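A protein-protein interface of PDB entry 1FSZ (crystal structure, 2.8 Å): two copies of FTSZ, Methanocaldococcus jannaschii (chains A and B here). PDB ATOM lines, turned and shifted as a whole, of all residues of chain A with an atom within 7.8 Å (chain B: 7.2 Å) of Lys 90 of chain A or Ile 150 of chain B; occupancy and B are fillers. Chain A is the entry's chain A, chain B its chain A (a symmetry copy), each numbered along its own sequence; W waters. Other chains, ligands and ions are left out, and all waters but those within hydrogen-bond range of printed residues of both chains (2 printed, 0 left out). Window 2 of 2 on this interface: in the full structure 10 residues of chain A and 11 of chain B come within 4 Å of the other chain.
The side-chain hydroxyl of Tyr 32 of chain B lies within hydrogen-bond range of the backbone carbonyl oxygen of Lys 89 of chain A (2.8 Å).
The side-chain amino group (NZ) of Lys 90 of chain A sits at hydrogen-bond distance from the backbone carbonyl oxygen (O) of Gln 120 of chain B.
O of Ile 150 of chain B sits at hydrogen-bond distance from NZ of Lys 90 of chain A, at 3.0 Å.
Of the 24 printed residues of chain B, 6 touch a printed residue of chain A.
Hydrophobic or aromatic side chains of chain B within 4 Å of the printed part of chain A: Tyr 32 and Ile 150.
Along chain B the printed residues that touch a printed residue of chain A span positions 32 to 240.
Of the 14 printed residues of chain A, 6 touch a printed residue of chain B.
Hydrophobic or aromatic side chains of chain A within 4 Å of the printed part of chain B: Leu 86.
Among the printed residues, no Asp or Glu carboxylate lies within 4 Å of a Lys or Arg side-chain nitrogen of the other chain.
Water W1 lies within hydrogen-bond range of the backbone carbonyl oxygen of Ile 150 of chain B (2.6 Å), the side-chain amino group of Lys 90 of chain A (2.7 Å), the side-chain amide nitrogen of Gln 120 of chain B (3.3 Å) and the backbone carbonyl oxygen of Glu 110 of chain A (3.3 Å).
Water W2 lies within hydrogen-bond range of O of Lys 90 of chain A (3.3 Å) and O of Asp 123 of chain B (3.5 Å).
OE2 of Glu 110 of chain A is in hydrogen-bond range of N of Lys 89 of chain A.
OE2 of Glu 110 of chain A sits at hydrogen-bond distance from N of Lys 90 of chain A, at 3.0 Å.
The backbone NH (N) of Leu 91 of chain A sits at hydrogen-bond distance from the side-chain carboxylate (OE1) of Glu 110 of chain A (3.0 Å).
O of Ile 119 of chain B lies within hydrogen-bond range of OG of Ser 122 of chain B, at 2.7 Å.
No position is printed for both chains.
Of the 10 pairs that touch across the chains among the printed residues, none has its exchanged pair printed and touching as well.
Printed residues of chain B within 4 Å of Lys 90 of chain A: Gln 120, Ser 122, Ile 150, Gly 151 and Lys 240.
Ile 150 of chain B touches just these residues of chain A: Lys 90 (3.0 Å) and Glu 110 (3.4 Å).
Of chain A, only Lys 90 (2.9 Å) comes within 4 Å of Gly 151 of chain B.
Printed residues of chain A within 4 Å of Ser 122 of chain B: Lys 90.
Of the printed residues of chain A, Tyr 32 of chain B touches Leu 86, Lys 89 and Arg 93.
Ile 119 of chain B touches none of the printed residues of chain A.
Glu 106 of chain A touches none of the printed residues of chain B.
The nearest residue of chain B that does not touch Lys 90 of chain A is Asp 123 of chain B (4.04 Å).
The nearest residue of chain A that does not touch Ile 150 of chain B is Glu 106 of chain A (6.1 Å).
The nearest printed residue of chain A that does not touch Lys 240 of chain B is Thr 92 of chain A (5.7 Å).
CD2 of Leu 86 of chain A touches CD2 of Tyr 32 of chain B, 3.6 Å away.
Lys 90 of chain A touches Ser 122 of chain B.
CD of Lys 90 of chain A touches O of Gly 151 of chain B, at 2.9 Å.
Lys 90 of chain A touches Lys 240 of chain B (O to NZ, 3.6 Å).
O of Leu 91 of chain A touches NZ of Lys 240 of chain B, at 3.7 Å.
Arg 93 of chain A touches Tyr 32 of chain B.
Ile 150 of chain B touches Glu 110 of chain A.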
ATOM      1  N   LEU A  86       7.131  11.869 -30.388  1.00  0.00           N
ATOM      2  CA  LEU A  86       5.718  11.534 -30.254  1.00  0.00           C
ATOM      3  C   LEU A  86       5.591  11.050 -28.826  1.00  0.00           C
ATOM      4  O   LEU A  86       6.020   9.932 -28.492  1.00  0.00           O
ATOM      5  CB  LEU A  86       5.323  10.426 -31.223  1.00  0.00           C
ATOM      6  CG  LEU A  86       3.847  10.030 -31.197  1.00  0.00           C
ATOM      7  CD1 LEU A  86       2.987  11.192 -31.686  1.00  0.00           C
ATOM      8  CD2 LEU A  86       3.662   8.807 -32.086  1.00  0.00           C
ATOM      9  N   ILE A  87       5.028  11.896 -27.967  1.00  0.00           N
ATOM     10  CA  ILE A  87       4.892  11.524 -26.559  1.00  0.00           C
ATOM     11  C   ILE A  87       3.531  10.889 -26.361  1.00  0.00           C
ATOM     12  O   ILE A  87       2.624  11.100 -27.165  1.00  0.00           O
ATOM     13  CB  ILE A  87       5.070  12.752 -25.597  1.00  0.00           C
ATOM     14  CG1 ILE A  87       4.085  13.843 -25.935  1.00  0.00           C
ATOM     15  CG2 ILE A  87       6.440  13.363 -25.772  1.00  0.00           C
ATOM     16  CD1 ILE A  87       3.716  14.620 -24.776  1.00  0.00           C
ATOM     17  N   GLY A  88       3.407  10.098 -25.303  1.00  0.00           N
ATOM     18  CA  GLY A  88       2.155   9.426 -25.011  1.00  0.00           C
ATOM     19  C   GLY A  88       1.859   8.274 -25.959  1.00  0.00           C
ATOM     20  O   GLY A  88       0.698   7.965 -26.230  1.00  0.00           O
ATOM     21  N   LYS A  89       2.905   7.631 -26.460  1.00  0.00           N
ATOM     22  CA  LYS A  89       2.746   6.523 -27.382  1.00  0.00           C
ATOM     23  C   LYS A  89       1.953   5.322 -26.836  1.00  0.00           C
ATOM     24  O   LYS A  89       1.355   4.580 -27.607  1.00  0.00           O
ATOM     25  CB  LYS A  89       4.114   6.044 -27.836  1.00  0.00           C
ATOM     26  CG  LYS A  89       4.551   6.672 -29.097  1.00  0.00           C
ATOM     27  CD  LYS A  89       5.469   5.732 -29.813  1.00  0.00           C
ATOM     28  CE  LYS A  89       6.915   6.056 -29.485  1.00  0.00           C
ATOM     29  NZ  LYS A  89       7.644   6.579 -30.685  1.00  0.00           N
ATOM     30  N   LYS A  90       1.958   5.094 -25.534  1.00  0.00           N
ATOM     31  CA  LYS A  90       1.225   3.962 -25.043  1.00  0.00           C
ATOM     32  C   LYS A  90      -0.117   4.441 -24.551  1.00  0.00           C
ATOM     33  O   LYS A  90      -1.137   3.786 -24.728  1.00  0.00           O
ATOM     34  CB  LYS A  90       1.991   3.310 -23.913  1.00  0.00           C
ATOM     35  CG  LYS A  90       3.305   2.741 -24.333  1.00  0.00           C
ATOM     36  CD  LYS A  90       4.082   2.237 -23.130  1.00  0.00           C
ATOM     37  CE  LYS A  90       5.474   1.771 -23.540  1.00  0.00           C
ATOM     38  NZ  LYS A  90       6.494   2.077 -22.482  1.00  0.00           N
ATOM     39  N   LEU A  91      -0.086   5.601 -23.912  1.00  0.00           N
ATOM     40  CA  LEU A  91      -1.267   6.269 -23.338  1.00  0.00           C
ATOM     41  C   LEU A  91      -2.275   6.616 -24.439  1.00  0.00           C
ATOM     42  O   LEU A  91      -3.402   6.149 -24.453  1.00  0.00           O
ATOM     43  CB  LEU A  91      -0.802   7.545 -22.648  1.00  0.00           C
ATOM     44  CG  LEU A  91      -1.958   8.356 -22.171  1.00  0.00           C
ATOM     45  CD1 LEU A  91      -2.958   7.450 -21.549  1.00  0.00           C
ATOM     46  CD2 LEU A  91      -1.454   9.317 -21.182  1.00  0.00           C
ATOM     47  N   THR A  92      -1.815   7.477 -25.331  1.00  0.00           N
ATOM     48  CA  THR A  92      -2.493   7.933 -26.530  1.00  0.00           C
ATOM     49  C   THR A  92      -1.952   6.873 -27.461  1.00  0.00           C
ATOM     50  O   THR A  92      -1.236   5.986 -26.993  1.00  0.00           O
ATOM     51  CB  THR A  92      -1.859   9.213 -26.951  1.00  0.00           C
ATOM     52  OG1 THR A  92      -2.309  10.254 -26.094  1.00  0.00           O
ATOM     53  CG2 THR A  92      -2.174   9.513 -28.355  1.00  0.00           C
ATOM     54  N   ARG A  93      -2.247   6.912 -28.750  1.00  0.00           N
ATOM     55  CA  ARG A  93      -1.614   5.903 -29.599  1.00  0.00           C
ATOM     56  C   ARG A  93      -1.123   6.602 -30.834  1.00  0.00           C
ATOM     57  O   ARG A  93      -1.052   6.014 -31.888  1.00  0.00           O
ATOM     58  CB  ARG A  93      -2.598   4.801 -29.990  1.00  0.00           C
ATOM     59  CG  ARG A  93      -2.727   3.644 -28.993  1.00  0.00           C
ATOM     60  CD  ARG A  93      -3.713   2.555 -29.488  1.00  0.00           C
ATOM     61  NE  ARG A  93      -5.113   3.008 -29.565  1.00  0.00           N
ATOM     62  CZ  ARG A  93      -6.093   2.363 -30.212  1.00  0.00           C
ATOM     63  NH1 ARG A  93      -5.837   1.221 -30.849  1.00  0.00           N
ATOM     64  NH2 ARG A  93      -7.335   2.855 -30.221  1.00  0.00           N
ATOM     65  N   GLY A  94      -0.801   7.878 -30.695  1.00  0.00           N
ATOM     66  CA  GLY A  94      -0.337   8.667 -31.824  1.00  0.00           C
ATOM     67  C   GLY A  94      -1.554   9.341 -32.417  1.00  0.00           C
ATOM     68  O   GLY A  94      -1.541   9.929 -33.514  1.00  0.00           O
ATOM     69  N   GLU A 106       0.240  12.914 -18.731  1.00  0.00           N
ATOM     70  CA  GLU A 106       0.732  11.538 -18.664  1.00  0.00           C
ATOM     71  C   GLU A 106       1.549  11.157 -19.907  1.00  0.00           C
ATOM     72  O   GLU A 106       2.564  10.452 -19.824  1.00  0.00           O
ATOM     73  CB  GLU A 106      -0.429  10.567 -18.474  1.00  0.00           C
ATOM     74  CG  GLU A 106      -0.216   9.589 -17.317  1.00  0.00           C
ATOM     75  CD  GLU A 106       0.658   8.360 -17.693  1.00  0.00           C
ATOM     76  OE1 GLU A 106       1.922   8.477 -17.759  1.00  0.00           O
ATOM     77  OE2 GLU A 106       0.062   7.268 -17.912  1.00  0.00           O
ATOM     78  N   ALA A 107       1.113  11.620 -21.066  1.00  0.00           N
ATOM     79  CA  ALA A 107       1.860  11.334 -22.262  1.00  0.00           C
ATOM     80  C   ALA A 107       3.274  11.845 -22.034  1.00  0.00           C
ATOM     81  O   ALA A 107       4.216  11.158 -22.340  1.00  0.00           O
ATOM     82  CB  ALA A 107       1.240  12.036 -23.434  1.00  0.00           C
ATOM     83  N   LYS A 109       4.784  12.578 -19.080  1.00  0.00           N
ATOM     84  CA  LYS A 109       5.412  11.913 -17.968  1.00  0.00           C
ATOM     85  C   LYS A 109       5.889  10.557 -18.455  1.00  0.00           C
ATOM     86  O   LYS A 109       6.961  10.095 -18.094  1.00  0.00           O
ATOM     87  CB  LYS A 109       4.422  11.752 -16.826  1.00  0.00           C
ATOM     88  CG  LYS A 109       4.474  12.862 -15.775  1.00  0.00           C
ATOM     89  CD  LYS A 109       3.185  12.908 -14.956  1.00  0.00           C
ATOM     90  CE  LYS A 109       3.437  12.888 -13.438  1.00  0.00           C
ATOM     91  NZ  LYS A 109       3.498  14.267 -12.810  1.00  0.00           N
ATOM     92  N   GLU A 110       5.090   9.933 -19.305  1.00  0.00           N
ATOM     93  CA  GLU A 110       5.420   8.629 -19.844  1.00  0.00           C
ATOM     94  C   GLU A 110       6.680   8.683 -20.734  1.00  0.00           C
ATOM     95  O   GLU A 110       7.419   7.701 -20.832  1.00  0.00           O
ATOM     96  CB  GLU A 110       4.200   8.114 -20.618  1.00  0.00           C
ATOM     97  CG  GLU A 110       4.341   6.723 -21.217  1.00  0.00           C
ATOM     98  CD  GLU A 110       3.391   6.490 -22.392  1.00  0.00           C
ATOM     99  OE1 GLU A 110       2.160   6.535 -22.173  1.00  0.00           O
ATOM    100  OE2 GLU A 110       3.874   6.262 -23.536  1.00  0.00           O
ATOM    101  N   SER A 111       6.931   9.832 -21.369  1.00  0.00           N
ATOM    102  CA  SER A 111       8.091  10.002 -22.246  1.00  0.00           C
ATOM    103  C   SER A 111       9.157  10.940 -21.678  1.00  0.00           C
ATOM    104  O   SER A 111       9.987  11.473 -22.420  1.00  0.00           O
ATOM    105  CB  SER A 111       7.660  10.537 -23.612  1.00  0.00           C
ATOM    106  OG  SER A 111       6.559   9.825 -24.148  1.00  0.00           O
ATOM    107  N   TYR B  32       4.958   3.951 -37.423  1.00  0.00           N
ATOM    108  CA  TYR B  32       4.357   3.766 -36.123  1.00  0.00           C
ATOM    109  C   TYR B  32       2.868   3.577 -36.227  1.00  0.00           C
ATOM    110  O   TYR B  32       2.318   2.663 -35.636  1.00  0.00           O
ATOM    111  CB  TYR B  32       4.645   4.953 -35.201  1.00  0.00           C
ATOM    112  CG  TYR B  32       3.988   4.768 -33.858  1.00  0.00           C
ATOM    113  CD1 TYR B  32       4.393   3.744 -32.997  1.00  0.00           C
ATOM    114  CD2 TYR B  32       2.911   5.572 -33.479  1.00  0.00           C
ATOM    115  CE1 TYR B  32       3.738   3.531 -31.798  1.00  0.00           C
ATOM    116  CE2 TYR B  32       2.245   5.377 -32.295  1.00  0.00           C
ATOM    117  CZ  TYR B  32       2.644   4.357 -31.451  1.00  0.00           C
ATOM    118  OH  TYR B  32       1.924   4.141 -30.277  1.00  0.00           O
ATOM    119  N   LYS B 116      13.822  -2.105 -16.438  1.00  0.00           N
ATOM    120  CA  LYS B 116      13.027  -1.165 -17.220  1.00  0.00           C
ATOM    121  C   LYS B 116      13.416  -1.139 -18.691  1.00  0.00           C
ATOM    122  O   LYS B 116      12.570  -0.994 -19.558  1.00  0.00           O
ATOM    123  CB  LYS B 116      13.148   0.233 -16.638  1.00  0.00           C
ATOM    124  CG  LYS B 116      12.837   1.323 -17.592  1.00  0.00           C
ATOM    125  CD  LYS B 116      13.990   2.308 -17.663  1.00  0.00           C
ATOM    126  CE  LYS B 116      13.538   3.746 -17.396  1.00  0.00           C
ATOM    127  NZ  LYS B 116      12.386   3.782 -16.446  1.00  0.00           N
ATOM    128  N   ALA B 117      14.698  -1.283 -18.962  1.00  0.00           N
ATOM    129  CA  ALA B 117      15.185  -1.268 -20.323  1.00  0.00           C
ATOM    130  C   ALA B 117      14.694  -2.470 -21.132  1.00  0.00           C
ATOM    131  O   ALA B 117      14.719  -2.451 -22.366  1.00  0.00           O
ATOM    132  CB  ALA B 117      16.683  -1.246 -20.303  1.00  0.00           C
ATOM    133  N   ALA B 118      14.243  -3.513 -20.440  1.00  0.00           N
ATOM    134  CA  ALA B 118      13.781  -4.736 -21.105  1.00  0.00           C
ATOM    135  C   ALA B 118      12.292  -4.714 -21.405  1.00  0.00           C
ATOM    136  O   ALA B 118      11.838  -5.369 -22.354  1.00  0.00           O
ATOM    137  CB  ALA B 118      14.106  -5.957 -20.244  1.00  0.00           C
ATOM    138  N   ILE B 119      11.532  -3.981 -20.592  1.00  0.00           N
ATOM    139  CA  ILE B 119      10.097  -3.899 -20.786  1.00  0.00           C
ATOM    140  C   ILE B 119       9.704  -2.533 -21.340  1.00  0.00           C
ATOM    141  O   ILE B 119       8.542  -2.248 -21.597  1.00  0.00           O
ATOM    142  CB  ILE B 119       9.342  -4.155 -19.466  1.00  0.00           C
ATOM    143  CG1 ILE B 119       9.631  -3.059 -18.459  1.00  0.00           C
ATOM    144  CG2 ILE B 119       9.762  -5.462 -18.860  1.00  0.00           C
ATOM    145  CD1 ILE B 119       8.834  -3.293 -17.188  1.00  0.00           C
ATOM    146  N   GLN B 120      10.708  -1.704 -21.542  1.00  0.00           N
ATOM    147  CA  GLN B 120      10.547  -0.354 -22.060  1.00  0.00           C
ATOM    148  C   GLN B 120       9.583  -0.110 -23.219  1.00  0.00           C
ATOM    149  O   GLN B 120       8.859   0.881 -23.213  1.00  0.00           O
ATOM    150  CB  GLN B 120      11.914   0.191 -22.481  1.00  0.00           C
ATOM    151  CG  GLN B 120      11.864   1.593 -22.990  1.00  0.00           C
ATOM    152  CD  GLN B 120      10.962   2.448 -22.135  1.00  0.00           C
ATOM    153  OE1 GLN B 120      11.155   2.530 -20.925  1.00  0.00           O
ATOM    154  NE2 GLN B 120       9.964   3.086 -22.753  1.00  0.00           N
ATOM    155  N   ASP B 121       9.559  -0.980 -24.220  1.00  0.00           N
ATOM    156  CA  ASP B 121       8.704  -0.694 -25.360  1.00  0.00           C
ATOM    157  C   ASP B 121       7.364  -1.404 -25.375  1.00  0.00           C
ATOM    158  O   ASP B 121       6.533  -1.192 -26.257  1.00  0.00           O
ATOM    159  CB  ASP B 121       9.489  -0.973 -26.633  1.00  0.00           C
ATOM    160  CG  ASP B 121      10.731  -0.058 -26.771  1.00  0.00           C
ATOM    161  OD1 ASP B 121      10.760   1.075 -26.201  1.00  0.00           O
ATOM    162  OD2 ASP B 121      11.690  -0.480 -27.460  1.00  0.00           O
ATOM    163  N   SER B 122       7.150  -2.231 -24.364  1.00  0.00           N
ATOM    164  CA  SER B 122       5.924  -2.993 -24.217  1.00  0.00           C
ATOM    165  C   SER B 122       4.713  -2.116 -24.033  1.00  0.00           C
ATOM    166  O   SER B 122       4.799  -1.075 -23.381  1.00  0.00           O
ATOM    167  CB  SER B 122       6.060  -3.896 -23.009  1.00  0.00           C
ATOM    168  OG  SER B 122       7.388  -4.338 -22.954  1.00  0.00           O
ATOM    169  N   ASP B 123       3.587  -2.563 -24.588  1.00  0.00           N
ATOM    170  CA  ASP B 123       2.309  -1.874 -24.479  1.00  0.00           C
ATOM    171  C   ASP B 123       1.624  -2.528 -23.303  1.00  0.00           C
ATOM    172  O   ASP B 123       0.805  -1.915 -22.624  1.00  0.00           O
ATOM    173  CB  ASP B 123       1.482  -2.099 -25.736  1.00  0.00           C
ATOM    174  CG  ASP B 123       1.806  -1.092 -26.849  1.00  0.00           C
ATOM    175  OD1 ASP B 123       1.409   0.104 -26.731  1.00  0.00           O
ATOM    176  OD2 ASP B 123       2.452  -1.500 -27.850  1.00  0.00           O
ATOM    177  N   MET B 124       1.977  -3.793 -23.090  1.00  0.00           N
ATOM    178  CA  MET B 124       1.465  -4.617 -21.993  1.00  0.00           C
ATOM    179  C   MET B 124       2.588  -5.481 -21.367  1.00  0.00           C
ATOM    180  O   MET B 124       3.427  -6.033 -22.078  1.00  0.00           O
ATOM    181  CB  MET B 124       0.346  -5.535 -22.503  1.00  0.00           C
ATOM    182  CG  MET B 124      -0.646  -5.958 -21.422  1.00  0.00           C
ATOM    183  SD  MET B 124      -1.866  -7.181 -21.960  1.00  0.00           S
ATOM    184  CE  MET B 124      -2.581  -7.602 -20.411  1.00  0.00           C
ATOM    185  N   VAL B 125       2.601  -5.602 -20.036  1.00  0.00           N
ATOM    186  CA  VAL B 125       3.620  -6.412 -19.354  1.00  0.00           C
ATOM    187  C   VAL B 125       2.953  -7.348 -18.355  1.00  0.00           C
ATOM    188  O   VAL B 125       2.103  -6.920 -17.572  1.00  0.00           O
ATOM    189  CB  VAL B 125       4.676  -5.542 -18.570  1.00  0.00           C
ATOM    190  CG1 VAL B 125       5.698  -6.459 -17.868  1.00  0.00           C
ATOM    191  CG2 VAL B 125       5.418  -4.604 -19.530  1.00  0.00           C
ATOM    192  N   ALA B 144       6.760  -4.544 -11.383  1.00  0.00           N
ATOM    193  CA  ALA B 144       5.414  -4.030 -11.630  1.00  0.00           C
ATOM    194  C   ALA B 144       5.325  -2.506 -11.531  1.00  0.00           C
ATOM    195  O   ALA B 144       4.715  -1.855 -12.367  1.00  0.00           O
ATOM    196  CB  ALA B 144       4.439  -4.667 -10.660  1.00  0.00           C
ATOM    197  N   GLU B 145       5.924  -1.935 -10.501  1.00  0.00           N
ATOM    198  CA  GLU B 145       5.902  -0.492 -10.344  1.00  0.00           C
ATOM    199  C   GLU B 145       6.721   0.210 -11.452  1.00  0.00           C
ATOM    200  O   GLU B 145       6.432   1.343 -11.855  1.00  0.00           O
ATOM    201  CB  GLU B 145       6.446  -0.150  -8.964  1.00  0.00           C
ATOM    202  CG  GLU B 145       7.211   1.148  -8.874  1.00  0.00           C
ATOM    203  CD  GLU B 145       7.633   1.462  -7.446  1.00  0.00           C
ATOM    204  OE1 GLU B 145       7.954   0.508  -6.686  1.00  0.00           O
ATOM    205  OE2 GLU B 145       7.639   2.665  -7.090  1.00  0.00           O
ATOM    206  N   ILE B 146       7.750  -0.475 -11.931  1.00  0.00           N
ATOM    207  CA  ILE B 146       8.615   0.039 -12.980  1.00  0.00           C
ATOM    208  C   ILE B 146       7.839   0.055 -14.277  1.00  0.00           C
ATOM    209  O   ILE B 146       7.957   0.986 -15.060  1.00  0.00           O
ATOM    210  CB  ILE B 146       9.837  -0.871 -13.174  1.00  0.00           C
ATOM    211  CG1 ILE B 146      10.739  -0.809 -11.944  1.00  0.00           C
ATOM    212  CG2 ILE B 146      10.564  -0.493 -14.436  1.00  0.00           C
ATOM    213  CD1 ILE B 146      11.965  -1.670 -12.086  1.00  0.00           C
ATOM    214  N   SER B 147       7.065  -1.007 -14.500  1.00  0.00           N
ATOM    215  CA  SER B 147       6.236  -1.159 -15.688  1.00  0.00           C
ATOM    216  C   SER B 147       5.174  -0.055 -15.728  1.00  0.00           C
ATOM    217  O   SER B 147       5.019   0.639 -16.729  1.00  0.00           O
ATOM    218  CB  SER B 147       5.568  -2.522 -15.654  1.00  0.00           C
ATOM    219  OG  SER B 147       4.728  -2.708 -16.770  1.00  0.00           O
ATOM    220  N   LYS B 148       4.452   0.108 -14.628  1.00  0.00           N
ATOM    221  CA  LYS B 148       3.424   1.133 -14.532  1.00  0.00           C
ATOM    222  C   LYS B 148       4.016   2.507 -14.830  1.00  0.00           C
ATOM    223  O   LYS B 148       3.382   3.328 -15.466  1.00  0.00           O
ATOM    224  CB  LYS B 148       2.800   1.112 -13.138  1.00  0.00           C
ATOM    225  CG  LYS B 148       1.607   0.178 -13.031  1.00  0.00           C
ATOM    226  CD  LYS B 148       0.277   0.942 -12.844  1.00  0.00           C
ATOM    227  CE  LYS B 148      -0.099   1.842 -14.053  1.00  0.00           C
ATOM    228  NZ  LYS B 148      -0.479   1.109 -15.326  1.00  0.00           N
ATOM    229  N   LYS B 149       5.234   2.757 -14.375  1.00  0.00           N
ATOM    230  CA  LYS B 149       5.879   4.036 -14.635  1.00  0.00           C
ATOM    231  C   LYS B 149       6.055   4.310 -16.130  1.00  0.00           C
ATOM    232  O   LYS B 149       5.847   5.431 -16.600  1.00  0.00           O
ATOM    233  CB  LYS B 149       7.252   4.082 -13.965  1.00  0.00           C
ATOM    234  CG  LYS B 149       7.270   4.860 -12.673  1.00  0.00           C
ATOM    235  CD  LYS B 149       8.586   5.617 -12.465  1.00  0.00           C
ATOM    236  CE  LYS B 149       9.354   5.131 -11.183  1.00  0.00           C
ATOM    237  NZ  LYS B 149       9.770   6.266 -10.232  1.00  0.00           N
ATOM    238  N   ILE B 150       6.445   3.294 -16.884  1.00  0.00           N
ATOM    239  CA  ILE B 150       6.656   3.486 -18.304  1.00  0.00           C
ATOM    240  C   ILE B 150       5.314   3.516 -19.010  1.00  0.00           C
ATOM    241  O   ILE B 150       5.221   3.582 -20.228  1.00  0.00           O
ATOM    242  CB  ILE B 150       7.580   2.384 -18.873  1.00  0.00           C
ATOM    243  CG1 ILE B 150       6.825   1.092 -19.092  1.00  0.00           C
ATOM    244  CG2 ILE B 150       8.687   2.089 -17.896  1.00  0.00           C
ATOM    245  CD1 ILE B 150       7.605   0.131 -19.926  1.00  0.00           C
ATOM    246  N   GLY B 151       4.263   3.482 -18.213  1.00  0.00           N
ATOM    247  CA  GLY B 151       2.931   3.524 -18.763  1.00  0.00           C
ATOM    248  C   GLY B 151       2.584   2.335 -19.623  1.00  0.00           C
ATOM    249  O   GLY B 151       2.305   2.481 -20.806  1.00  0.00           O
ATOM    250  N   ALA B 152       2.592   1.154 -19.022  1.00  0.00           N
ATOM    251  CA  ALA B 152       2.247  -0.067 -19.731  1.00  0.00           C
ATOM    252  C   ALA B 152       1.112  -0.741 -18.965  1.00  0.00           C
ATOM    253  O   ALA B 152       0.785  -0.363 -17.837  1.00  0.00           O
ATOM    254  CB  ALA B 152       3.448  -0.979 -19.812  1.00  0.00           C
ATOM    255  N   LEU B 153       0.479  -1.720 -19.582  1.00  0.00           N
ATOM    256  CA  LEU B 153      -0.600  -2.390 -18.895  1.00  0.00           C
ATOM    257  C   LEU B 153       0.050  -3.444 -18.014  1.00  0.00           C
ATOM    258  O   LEU B 153       0.540  -4.478 -18.474  1.00  0.00           O
ATOM    259  CB  LEU B 153      -1.566  -3.015 -19.906  1.00  0.00           C
ATOM    260  CG  LEU B 153      -3.080  -3.096 -19.633  1.00  0.00           C
ATOM    261  CD1 LEU B 153      -3.537  -4.472 -20.092  1.00  0.00           C
ATOM    262  CD2 LEU B 153      -3.444  -2.877 -18.162  1.00  0.00           C
ATOM    263  N   THR B 154       0.051  -3.165 -16.728  1.00  0.00           N
ATOM    264  CA  THR B 154       0.667  -4.058 -15.786  1.00  0.00           C
ATOM    265  C   THR B 154      -0.246  -5.108 -15.225  1.00  0.00           C
ATOM    266  O   THR B 154      -1.138  -4.819 -14.434  1.00  0.00           O
ATOM    267  CB  THR B 154       1.247  -3.274 -14.653  1.00  0.00           C
ATOM    268  OG1 THR B 154       1.976  -2.177 -15.200  1.00  0.00           O
ATOM    269  CG2 THR B 154       2.178  -4.114 -13.860  1.00  0.00           C
ATOM    270  N   PHE B 236      -7.533  -4.475 -28.218  1.00  0.00           N
ATOM    271  CA  PHE B 236      -6.593  -4.205 -27.138  1.00  0.00           C
ATOM    272  C   PHE B 236      -7.044  -2.995 -26.343  1.00  0.00           C
ATOM    273  O   PHE B 236      -6.800  -2.890 -25.133  1.00  0.00           O
ATOM    274  CB  PHE B 236      -5.189  -3.952 -27.680  1.00  0.00           C
ATOM    275  CG  PHE B 236      -4.149  -3.795 -26.602  1.00  0.00           C
ATOM    276  CD1 PHE B 236      -3.519  -4.904 -26.058  1.00  0.00           C
ATOM    277  CD2 PHE B 236      -3.845  -2.544 -26.082  1.00  0.00           C
ATOM    278  CE1 PHE B 236      -2.613  -4.757 -25.020  1.00  0.00           C
ATOM    279  CE2 PHE B 236      -2.940  -2.398 -25.039  1.00  0.00           C
ATOM    280  CZ  PHE B 236      -2.332  -3.500 -24.512  1.00  0.00           C
ATOM    281  N   LYS B 240      -7.310  -3.148 -22.298  1.00  0.00           N
ATOM    282  CA  LYS B 240      -6.697  -2.117 -21.472  1.00  0.00           C
ATOM    283  C   LYS B 240      -7.728  -1.440 -20.586  1.00  0.00           C
ATOM    284  O   LYS B 240      -7.447  -1.085 -19.457  1.00  0.00           O
ATOM    285  CB  LYS B 240      -5.990  -1.092 -22.377  1.00  0.00           C
ATOM    286  CG  LYS B 240      -5.453   0.161 -21.669  1.00  0.00           C
ATOM    287  CD  LYS B 240      -4.013   0.479 -22.120  1.00  0.00           C
ATOM    288  CE  LYS B 240      -3.505   1.853 -21.628  1.00  0.00           C
ATOM    289  NZ  LYS B 240      -3.853   2.981 -22.582  1.00  0.00           N
HETATM  290  O   HOH W   1       7.284   4.495 -21.559  1.00  0.00           O
HETATM  291  O   HOH W   2      -1.240   0.738 -23.602  1.00  0.00           O
